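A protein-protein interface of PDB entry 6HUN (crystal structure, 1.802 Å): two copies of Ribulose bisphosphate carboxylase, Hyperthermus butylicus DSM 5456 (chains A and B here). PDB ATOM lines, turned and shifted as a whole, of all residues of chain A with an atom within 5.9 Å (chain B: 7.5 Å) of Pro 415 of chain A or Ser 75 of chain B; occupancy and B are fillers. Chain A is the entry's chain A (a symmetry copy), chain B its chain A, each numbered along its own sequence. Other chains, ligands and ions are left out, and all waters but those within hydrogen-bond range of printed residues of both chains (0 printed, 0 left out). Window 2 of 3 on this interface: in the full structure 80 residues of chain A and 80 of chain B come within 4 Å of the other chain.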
ATOM      1  N   TYR A 182       7.159  -7.762 -11.698  1.00  0.00           N
ATOM      2  CA  TYR A 182       8.251  -8.632 -12.111  1.00  0.00           C
ATOM      3  C   TYR A 182       9.419  -7.815 -12.667  1.00  0.00           C
ATOM      4  O   TYR A 182       9.225  -6.879 -13.453  1.00  0.00           O
ATOM      5  CB  TYR A 182       7.751  -9.625 -13.177  1.00  0.00           C
ATOM      6  CG  TYR A 182       6.798 -10.690 -12.657  1.00  0.00           C
ATOM      7  CD1 TYR A 182       7.239 -11.638 -11.737  1.00  0.00           C
ATOM      8  CD2 TYR A 182       5.463 -10.742 -13.076  1.00  0.00           C
ATOM      9  CE1 TYR A 182       6.391 -12.611 -11.248  1.00  0.00           C
ATOM     10  CE2 TYR A 182       4.589 -11.722 -12.582  1.00  0.00           C
ATOM     11  CZ  TYR A 182       5.066 -12.652 -11.667  1.00  0.00           C
ATOM     12  OH  TYR A 182       4.256 -13.649 -11.145  1.00  0.00           O
ATOM     13  N   VAL A 190       8.422 -16.408 -16.022  1.00  0.00           N
ATOM     14  CA  VAL A 190       6.966 -16.583 -16.026  1.00  0.00           C
ATOM     15  C   VAL A 190       6.462 -16.892 -17.431  1.00  0.00           C
ATOM     16  O   VAL A 190       5.579 -17.745 -17.619  1.00  0.00           O
ATOM     17  CB  VAL A 190       6.256 -15.340 -15.441  1.00  0.00           C
ATOM     18  CG1 VAL A 190       4.734 -15.509 -15.479  1.00  0.00           C
ATOM     19  CG2 VAL A 190       6.701 -15.088 -14.007  1.00  0.00           C
ATOM     20  N   GLU A 193       7.060 -20.650 -18.692  1.00  0.00           N
ATOM     21  CA  GLU A 193       6.122 -21.682 -18.247  1.00  0.00           C
ATOM     22  C   GLU A 193       4.809 -21.612 -19.019  1.00  0.00           C
ATOM     23  O   GLU A 193       4.230 -22.654 -19.370  1.00  0.00           O
ATOM     24  CB  GLU A 193       5.861 -21.533 -16.752  1.00  0.00           C
ATOM     25  CG  GLU A 193       7.087 -21.115 -15.988  1.00  0.00           C
ATOM     26  CD  GLU A 193       7.042 -21.537 -14.540  1.00  0.00           C
ATOM     27  OE1 GLU A 193       6.540 -20.748 -13.712  1.00  0.00           O
ATOM     28  OE2 GLU A 193       7.517 -22.653 -14.234  1.00  0.00           O
ATOM     29  N   ILE A 194       4.331 -20.390 -19.285  1.00  0.00           N
ATOM     30  CA  ILE A 194       3.103 -20.179 -20.056  1.00  0.00           C
ATOM     31  C   ILE A 194       3.234 -20.814 -21.444  1.00  0.00           C
ATOM     32  O   ILE A 194       2.433 -21.668 -21.832  1.00  0.00           O
ATOM     33  CB  ILE A 194       2.783 -18.670 -20.128  1.00  0.00           C
ATOM     34  CG1 ILE A 194       2.262 -18.166 -18.768  1.00  0.00           C
ATOM     35  CG2 ILE A 194       1.756 -18.328 -21.226  1.00  0.00           C
ATOM     36  CD1 ILE A 194       2.439 -16.672 -18.528  1.00  0.00           C
ATOM     37  N   GLY A 197       3.777 -24.885 -22.013  1.00  0.00           N
ATOM     38  CA  GLY A 197       2.685 -25.828 -21.933  1.00  0.00           C
ATOM     39  C   GLY A 197       1.618 -25.733 -23.004  1.00  0.00           C
ATOM     40  O   GLY A 197       0.659 -26.501 -22.952  1.00  0.00           O
ATOM     41  N   VAL A 408      -5.107 -20.807 -16.624  1.00  0.00           N
ATOM     42  CA  VAL A 408      -3.762 -21.310 -16.885  1.00  0.00           C
ATOM     43  C   VAL A 408      -2.878 -21.200 -15.655  1.00  0.00           C
ATOM     44  O   VAL A 408      -2.312 -22.197 -15.187  1.00  0.00           O
ATOM     45  CB  VAL A 408      -3.150 -20.557 -18.089  1.00  0.00           C
ATOM     46  CG1 VAL A 408      -1.618 -20.685 -18.093  1.00  0.00           C
ATOM     47  CG2 VAL A 408      -3.723 -21.080 -19.382  1.00  0.00           C
ATOM     48  N   LEU A 409      -2.752 -19.992 -15.105  1.00  0.00           N
ATOM     49  CA  LEU A 409      -1.868 -19.742 -13.974  1.00  0.00           C
ATOM     50  C   LEU A 409      -2.404 -20.310 -12.667  1.00  0.00           C
ATOM     51  O   LEU A 409      -1.627 -20.495 -11.724  1.00  0.00           O
ATOM     52  CB  LEU A 409      -1.624 -18.228 -13.862  1.00  0.00           C
ATOM     53  CG  LEU A 409      -1.359 -17.628 -15.223  1.00  0.00           C
ATOM     54  CD1 LEU A 409      -1.490 -16.092 -15.218  1.00  0.00           C
ATOM     55  CD2 LEU A 409       0.019 -18.016 -15.641  1.00  0.00           C
ATOM     56  N   HIS A 411      -3.909 -23.396 -12.331  1.00  0.00           N
ATOM     57  CA  HIS A 411      -4.086 -24.854 -12.369  1.00  0.00           C
ATOM     58  C   HIS A 411      -3.355 -25.523 -11.202  1.00  0.00           C
ATOM     59  O   HIS A 411      -2.208 -25.181 -10.902  1.00  0.00           O
ATOM     60  CB  HIS A 411      -3.581 -25.419 -13.698  1.00  0.00           C
ATOM     61  CG  HIS A 411      -4.036 -26.822 -13.988  1.00  0.00           C
ATOM     62  ND1 HIS A 411      -3.241 -27.928 -13.756  1.00  0.00           N
ATOM     63  CD2 HIS A 411      -5.192 -27.297 -14.511  1.00  0.00           C
ATOM     64  CE1 HIS A 411      -3.892 -29.022 -14.109  1.00  0.00           C
ATOM     65  NE2 HIS A 411      -5.081 -28.671 -14.566  1.00  0.00           N
ATOM     66  N   ASP A 413      -1.636 -28.023 -10.809  1.00  0.00           N
ATOM     67  CA  ASP A 413      -0.340 -28.605 -11.136  1.00  0.00           C
ATOM     68  C   ASP A 413       0.613 -27.614 -11.788  1.00  0.00           C
ATOM     69  O   ASP A 413       1.593 -28.037 -12.418  1.00  0.00           O
ATOM     70  CB  ASP A 413      -0.506 -29.812 -12.056  1.00  0.00           C
ATOM     71  CG  ASP A 413      -1.260 -30.942 -11.398  1.00  0.00           C
ATOM     72  OD1 ASP A 413      -2.293 -31.377 -11.953  1.00  0.00           O
ATOM     73  OD2 ASP A 413      -0.827 -31.376 -10.308  1.00  0.00           O
ATOM     74  N   GLY A 414       0.350 -26.316 -11.680  1.00  0.00           N
ATOM     75  CA  GLY A 414       1.253 -25.350 -12.238  1.00  0.00           C
ATOM     76  C   GLY A 414       0.838 -24.926 -13.632  1.00  0.00           C
ATOM     77  O   GLY A 414      -0.023 -25.545 -14.273  1.00  0.00           O
ATOM     78  N   PRO A 415       1.451 -23.853 -14.131  1.00  0.00           N
ATOM     79  CA  PRO A 415       0.939 -23.241 -15.371  1.00  0.00           C
ATOM     80  C   PRO A 415       1.172 -24.085 -16.613  1.00  0.00           C
ATOM     81  O   PRO A 415       0.309 -24.112 -17.498  1.00  0.00           O
ATOM     82  CB  PRO A 415       1.686 -21.899 -15.434  1.00  0.00           C
ATOM     83  CG  PRO A 415       2.898 -22.093 -14.563  1.00  0.00           C
ATOM     84  CD  PRO A 415       2.479 -23.029 -13.476  1.00  0.00           C
ATOM     85  N   GLU A 416       2.312 -24.775 -16.701  1.00  0.00           N
ATOM     86  CA  GLU A 416       2.546 -25.696 -17.807  1.00  0.00           C
ATOM     87  C   GLU A 416       1.367 -26.649 -17.979  1.00  0.00           C
ATOM     88  O   GLU A 416       0.735 -26.692 -19.044  1.00  0.00           O
ATOM     89  CB  GLU A 416       3.849 -26.457 -17.570  1.00  0.00           C
ATOM     90  CG  GLU A 416       4.992 -25.558 -17.089  1.00  0.00           C
ATOM     91  CD  GLU A 416       5.050 -25.406 -15.561  1.00  0.00           C
ATOM     92  OE1 GLU A 416       6.168 -25.311 -15.004  1.00  0.00           O
ATOM     93  OE2 GLU A 416       3.978 -25.366 -14.920  1.00  0.00           O
ATOM     94  N   ALA A 417       1.026 -27.379 -16.913  1.00  0.00           N
ATOM     95  CA  ALA A 417      -0.166 -28.222 -16.932  1.00  0.00           C
ATOM     96  C   ALA A 417      -1.428 -27.405 -17.197  1.00  0.00           C
ATOM     97  O   ALA A 417      -2.332 -27.862 -17.904  1.00  0.00           O
ATOM     98  CB  ALA A 417      -0.284 -28.990 -15.616  1.00  0.00           C
ATOM     99  N   GLY A 418      -1.503 -26.186 -16.652  1.00  0.00           N
ATOM    100  CA  GLY A 418      -2.652 -25.330 -16.934  1.00  0.00           C
ATOM    101  C   GLY A 418      -2.817 -25.002 -18.409  1.00  0.00           C
ATOM    102  O   GLY A 418      -3.927 -25.036 -18.938  1.00  0.00           O
ATOM    103  N   ALA A 419      -1.725 -24.656 -19.091  1.00  0.00           N
ATOM    104  CA  ALA A 419      -1.826 -24.432 -20.531  1.00  0.00           C
ATOM    105  C   ALA A 419      -2.204 -25.726 -21.257  1.00  0.00           C
ATOM    106  O   ALA A 419      -2.963 -25.708 -22.235  1.00  0.00           O
ATOM    107  CB  ALA A 419      -0.518 -23.866 -21.060  1.00  0.00           C
ATOM    108  N   ARG A 420      -1.719 -26.869 -20.769  1.00  0.00           N
ATOM    109  CA  ARG A 420      -2.092 -28.116 -21.429  1.00  0.00           C
ATOM    110  C   ARG A 420      -3.579 -28.404 -21.249  1.00  0.00           C
ATOM    111  O   ARG A 420      -4.250 -28.852 -22.191  1.00  0.00           O
ATOM    112  CB  ARG A 420      -1.245 -29.281 -20.916  1.00  0.00           C
ATOM    113  CG  ARG A 420      -0.820 -30.182 -22.045  1.00  0.00           C
ATOM    114  CD  ARG A 420       0.554 -30.752 -21.774  1.00  0.00           C
ATOM    115  NE  ARG A 420       0.680 -31.153 -20.372  1.00  0.00           N
ATOM    116  CZ  ARG A 420       1.577 -30.638 -19.536  1.00  0.00           C
ATOM    117  NH1 ARG A 420       2.445 -29.726 -19.976  1.00  0.00           N
ATOM    118  NH2 ARG A 420       1.614 -31.047 -18.270  1.00  0.00           N
ATOM    119  N   TRP B  71      -2.967 -11.889  -7.607  1.00  0.00           N
ATOM    120  CA  TRP B  71      -2.433 -13.200  -7.942  1.00  0.00           C
ATOM    121  C   TRP B  71      -3.122 -14.230  -7.071  1.00  0.00           C
ATOM    122  O   TRP B  71      -3.573 -13.925  -5.961  1.00  0.00           O
ATOM    123  CB  TRP B  71      -0.900 -13.252  -7.778  1.00  0.00           C
ATOM    124  CG  TRP B  71      -0.411 -13.718  -6.429  1.00  0.00           C
ATOM    125  CD1 TRP B  71      -0.260 -15.003  -6.010  1.00  0.00           C
ATOM    126  CD2 TRP B  71      -0.016 -12.888  -5.328  1.00  0.00           C
ATOM    127  NE1 TRP B  71       0.206 -15.030  -4.717  1.00  0.00           N
ATOM    128  CE2 TRP B  71       0.364 -13.744  -4.275  1.00  0.00           C
ATOM    129  CE3 TRP B  71       0.044 -11.504  -5.129  1.00  0.00           C
ATOM    130  CZ2 TRP B  71       0.811 -13.267  -3.038  1.00  0.00           C
ATOM    131  CZ3 TRP B  71       0.496 -11.035  -3.888  1.00  0.00           C
ATOM    132  CH2 TRP B  71       0.870 -11.915  -2.866  1.00  0.00           C
ATOM    133  N   THR B  73      -1.655 -17.933  -7.122  1.00  0.00           N
ATOM    134  CA  THR B  73      -0.423 -18.615  -6.721  1.00  0.00           C
ATOM    135  C   THR B  73       0.744 -18.001  -7.491  1.00  0.00           C
ATOM    136  O   THR B  73       0.567 -17.469  -8.590  1.00  0.00           O
ATOM    137  CB  THR B  73      -0.508 -20.150  -6.957  1.00  0.00           C
ATOM    138  OG1 THR B  73       0.496 -20.816  -6.184  1.00  0.00           O
ATOM    139  CG2 THR B  73      -0.324 -20.490  -8.428  1.00  0.00           C
ATOM    140  N   LEU B  74       1.932 -18.032  -6.896  1.00  0.00           N
ATOM    141  CA  LEU B  74       3.108 -17.397  -7.485  1.00  0.00           C
ATOM    142  C   LEU B  74       4.082 -18.467  -7.964  1.00  0.00           C
ATOM    143  O   LEU B  74       4.628 -19.218  -7.149  1.00  0.00           O
ATOM    144  CB  LEU B  74       3.801 -16.477  -6.486  1.00  0.00           C
ATOM    145  CG  LEU B  74       3.294 -15.045  -6.446  1.00  0.00           C
ATOM    146  CD1 LEU B  74       4.067 -14.242  -5.413  1.00  0.00           C
ATOM    147  CD2 LEU B  74       3.357 -14.434  -7.838  1.00  0.00           C
ATOM    148  N   SER B  75       4.315 -18.513  -9.280  1.00  0.00           N
ATOM    149  CA  SER B  75       5.296 -19.422  -9.866  1.00  0.00           C
ATOM    150  C   SER B  75       6.664 -18.775 -10.076  1.00  0.00           C
ATOM    151  O   SER B  75       7.625 -19.483 -10.386  1.00  0.00           O
ATOM    152  CB  SER B  75       4.771 -19.982 -11.195  1.00  0.00           C
ATOM    153  OG  SER B  75       3.861 -21.049 -10.964  1.00  0.00           O
ATOM    154  N   VAL B  76       6.764 -17.460  -9.921  1.00  0.00           N
ATOM    155  CA  VAL B  76       8.023 -16.721  -9.855  1.00  0.00           C
ATOM    156  C   VAL B  76       7.741 -15.476  -9.018  1.00  0.00           C
ATOM    157  O   VAL B  76       6.680 -14.863  -9.150  1.00  0.00           O
ATOM    158  CB  VAL B  76       8.560 -16.371 -11.269  1.00  0.00           C
ATOM    159  CG1 VAL B  76       9.513 -15.188 -11.221  1.00  0.00           C
ATOM    160  CG2 VAL B  76       9.259 -17.584 -11.927  1.00  0.00           C
ATOM    161  N   LYS B  77       8.644 -15.144  -8.103  1.00  0.00           N
ATOM    162  CA  LYS B  77       8.367 -14.038  -7.191  1.00  0.00           C
ATOM    163  C   LYS B  77       8.336 -12.726  -7.964  1.00  0.00           C
ATOM    164  O   LYS B  77       9.242 -12.475  -8.767  1.00  0.00           O
ATOM    165  CB  LYS B  77       9.420 -13.961  -6.090  1.00  0.00           C
ATOM    166  CG  LYS B  77       9.708 -12.558  -5.583  1.00  0.00           C
ATOM    167  CD  LYS B  77      10.333 -12.545  -4.194  1.00  0.00           C
ATOM    168  CE  LYS B  77      11.286 -11.365  -3.998  1.00  0.00           C
ATOM    169  NZ  LYS B  77      12.504 -11.425  -4.862  1.00  0.00           N
ATOM    170  N   PRO B  78       7.295 -11.866  -7.770  1.00  0.00           N
ATOM    171  CA  PRO B  78       7.387 -10.480  -8.240  1.00  0.00           C
ATOM    172  C   PRO B  78       7.973  -9.599  -7.147  1.00  0.00           C
ATOM    173  O   PRO B  78       7.281  -9.237  -6.186  1.00  0.00           O
ATOM    174  CB  PRO B  78       5.930 -10.116  -8.565  1.00  0.00           C
ATOM    175  CG  PRO B  78       5.077 -11.107  -7.763  1.00  0.00           C
ATOM    176  CD  PRO B  78       6.003 -12.119  -7.114  1.00  0.00           C
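Among the printed residues, merely in contact across the chains: Glu 193 of chain A with Ser 75 of chain B, Pro 415 of chain A with Ser 75 of chain B, Tyr 182 of chain A with Leu 74 of chain B, Leu 409 of chain A with Thr 73 of chain B, Val 190 of chain A with Val 76 of chain B, Tyr 182 of chain A with Pro 78 of chain B and Tyr 182 of chain A with Lys 77 of chain B.
Hydrophobic or aromatic side chains of chain A within 4 Å of the printed part of chain B: Tyr 182, Val 190 and Pro 415. Hydrophobic or aromatic side chains of chain B within 4 Å of the printed part of chain A: Leu 74, Val 76 and Pro 78. Among the printed residues, no Asp or Glu carboxylate lies within 4 Å of a Lys or Arg side-chain nitrogen of the other chain.
Pro 415 of chain A touches one residue of chain B. Ser 75 of chain B touches just these residues of chain A: Glu 193 and Pro 415. Of the printed residues of chain B, Leu 409 of chain A touches Thr 73. Printed residues of chain B within 4 Å of Glu 193 of chain A: Ser 75. Glu 416 of chain A touches none of the printed residues of chain B. Ala 417 of chain A touches none of the printed residues of chain B. The nearest printed residue of chain A that does not touch Ser 75 of chain B is Gly 414 of chain A (5.2 Å).
No position is printed for both chains.
O of Val 76 of chain B sits close to OH of Tyr 182 of chain A (3.4 Å).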
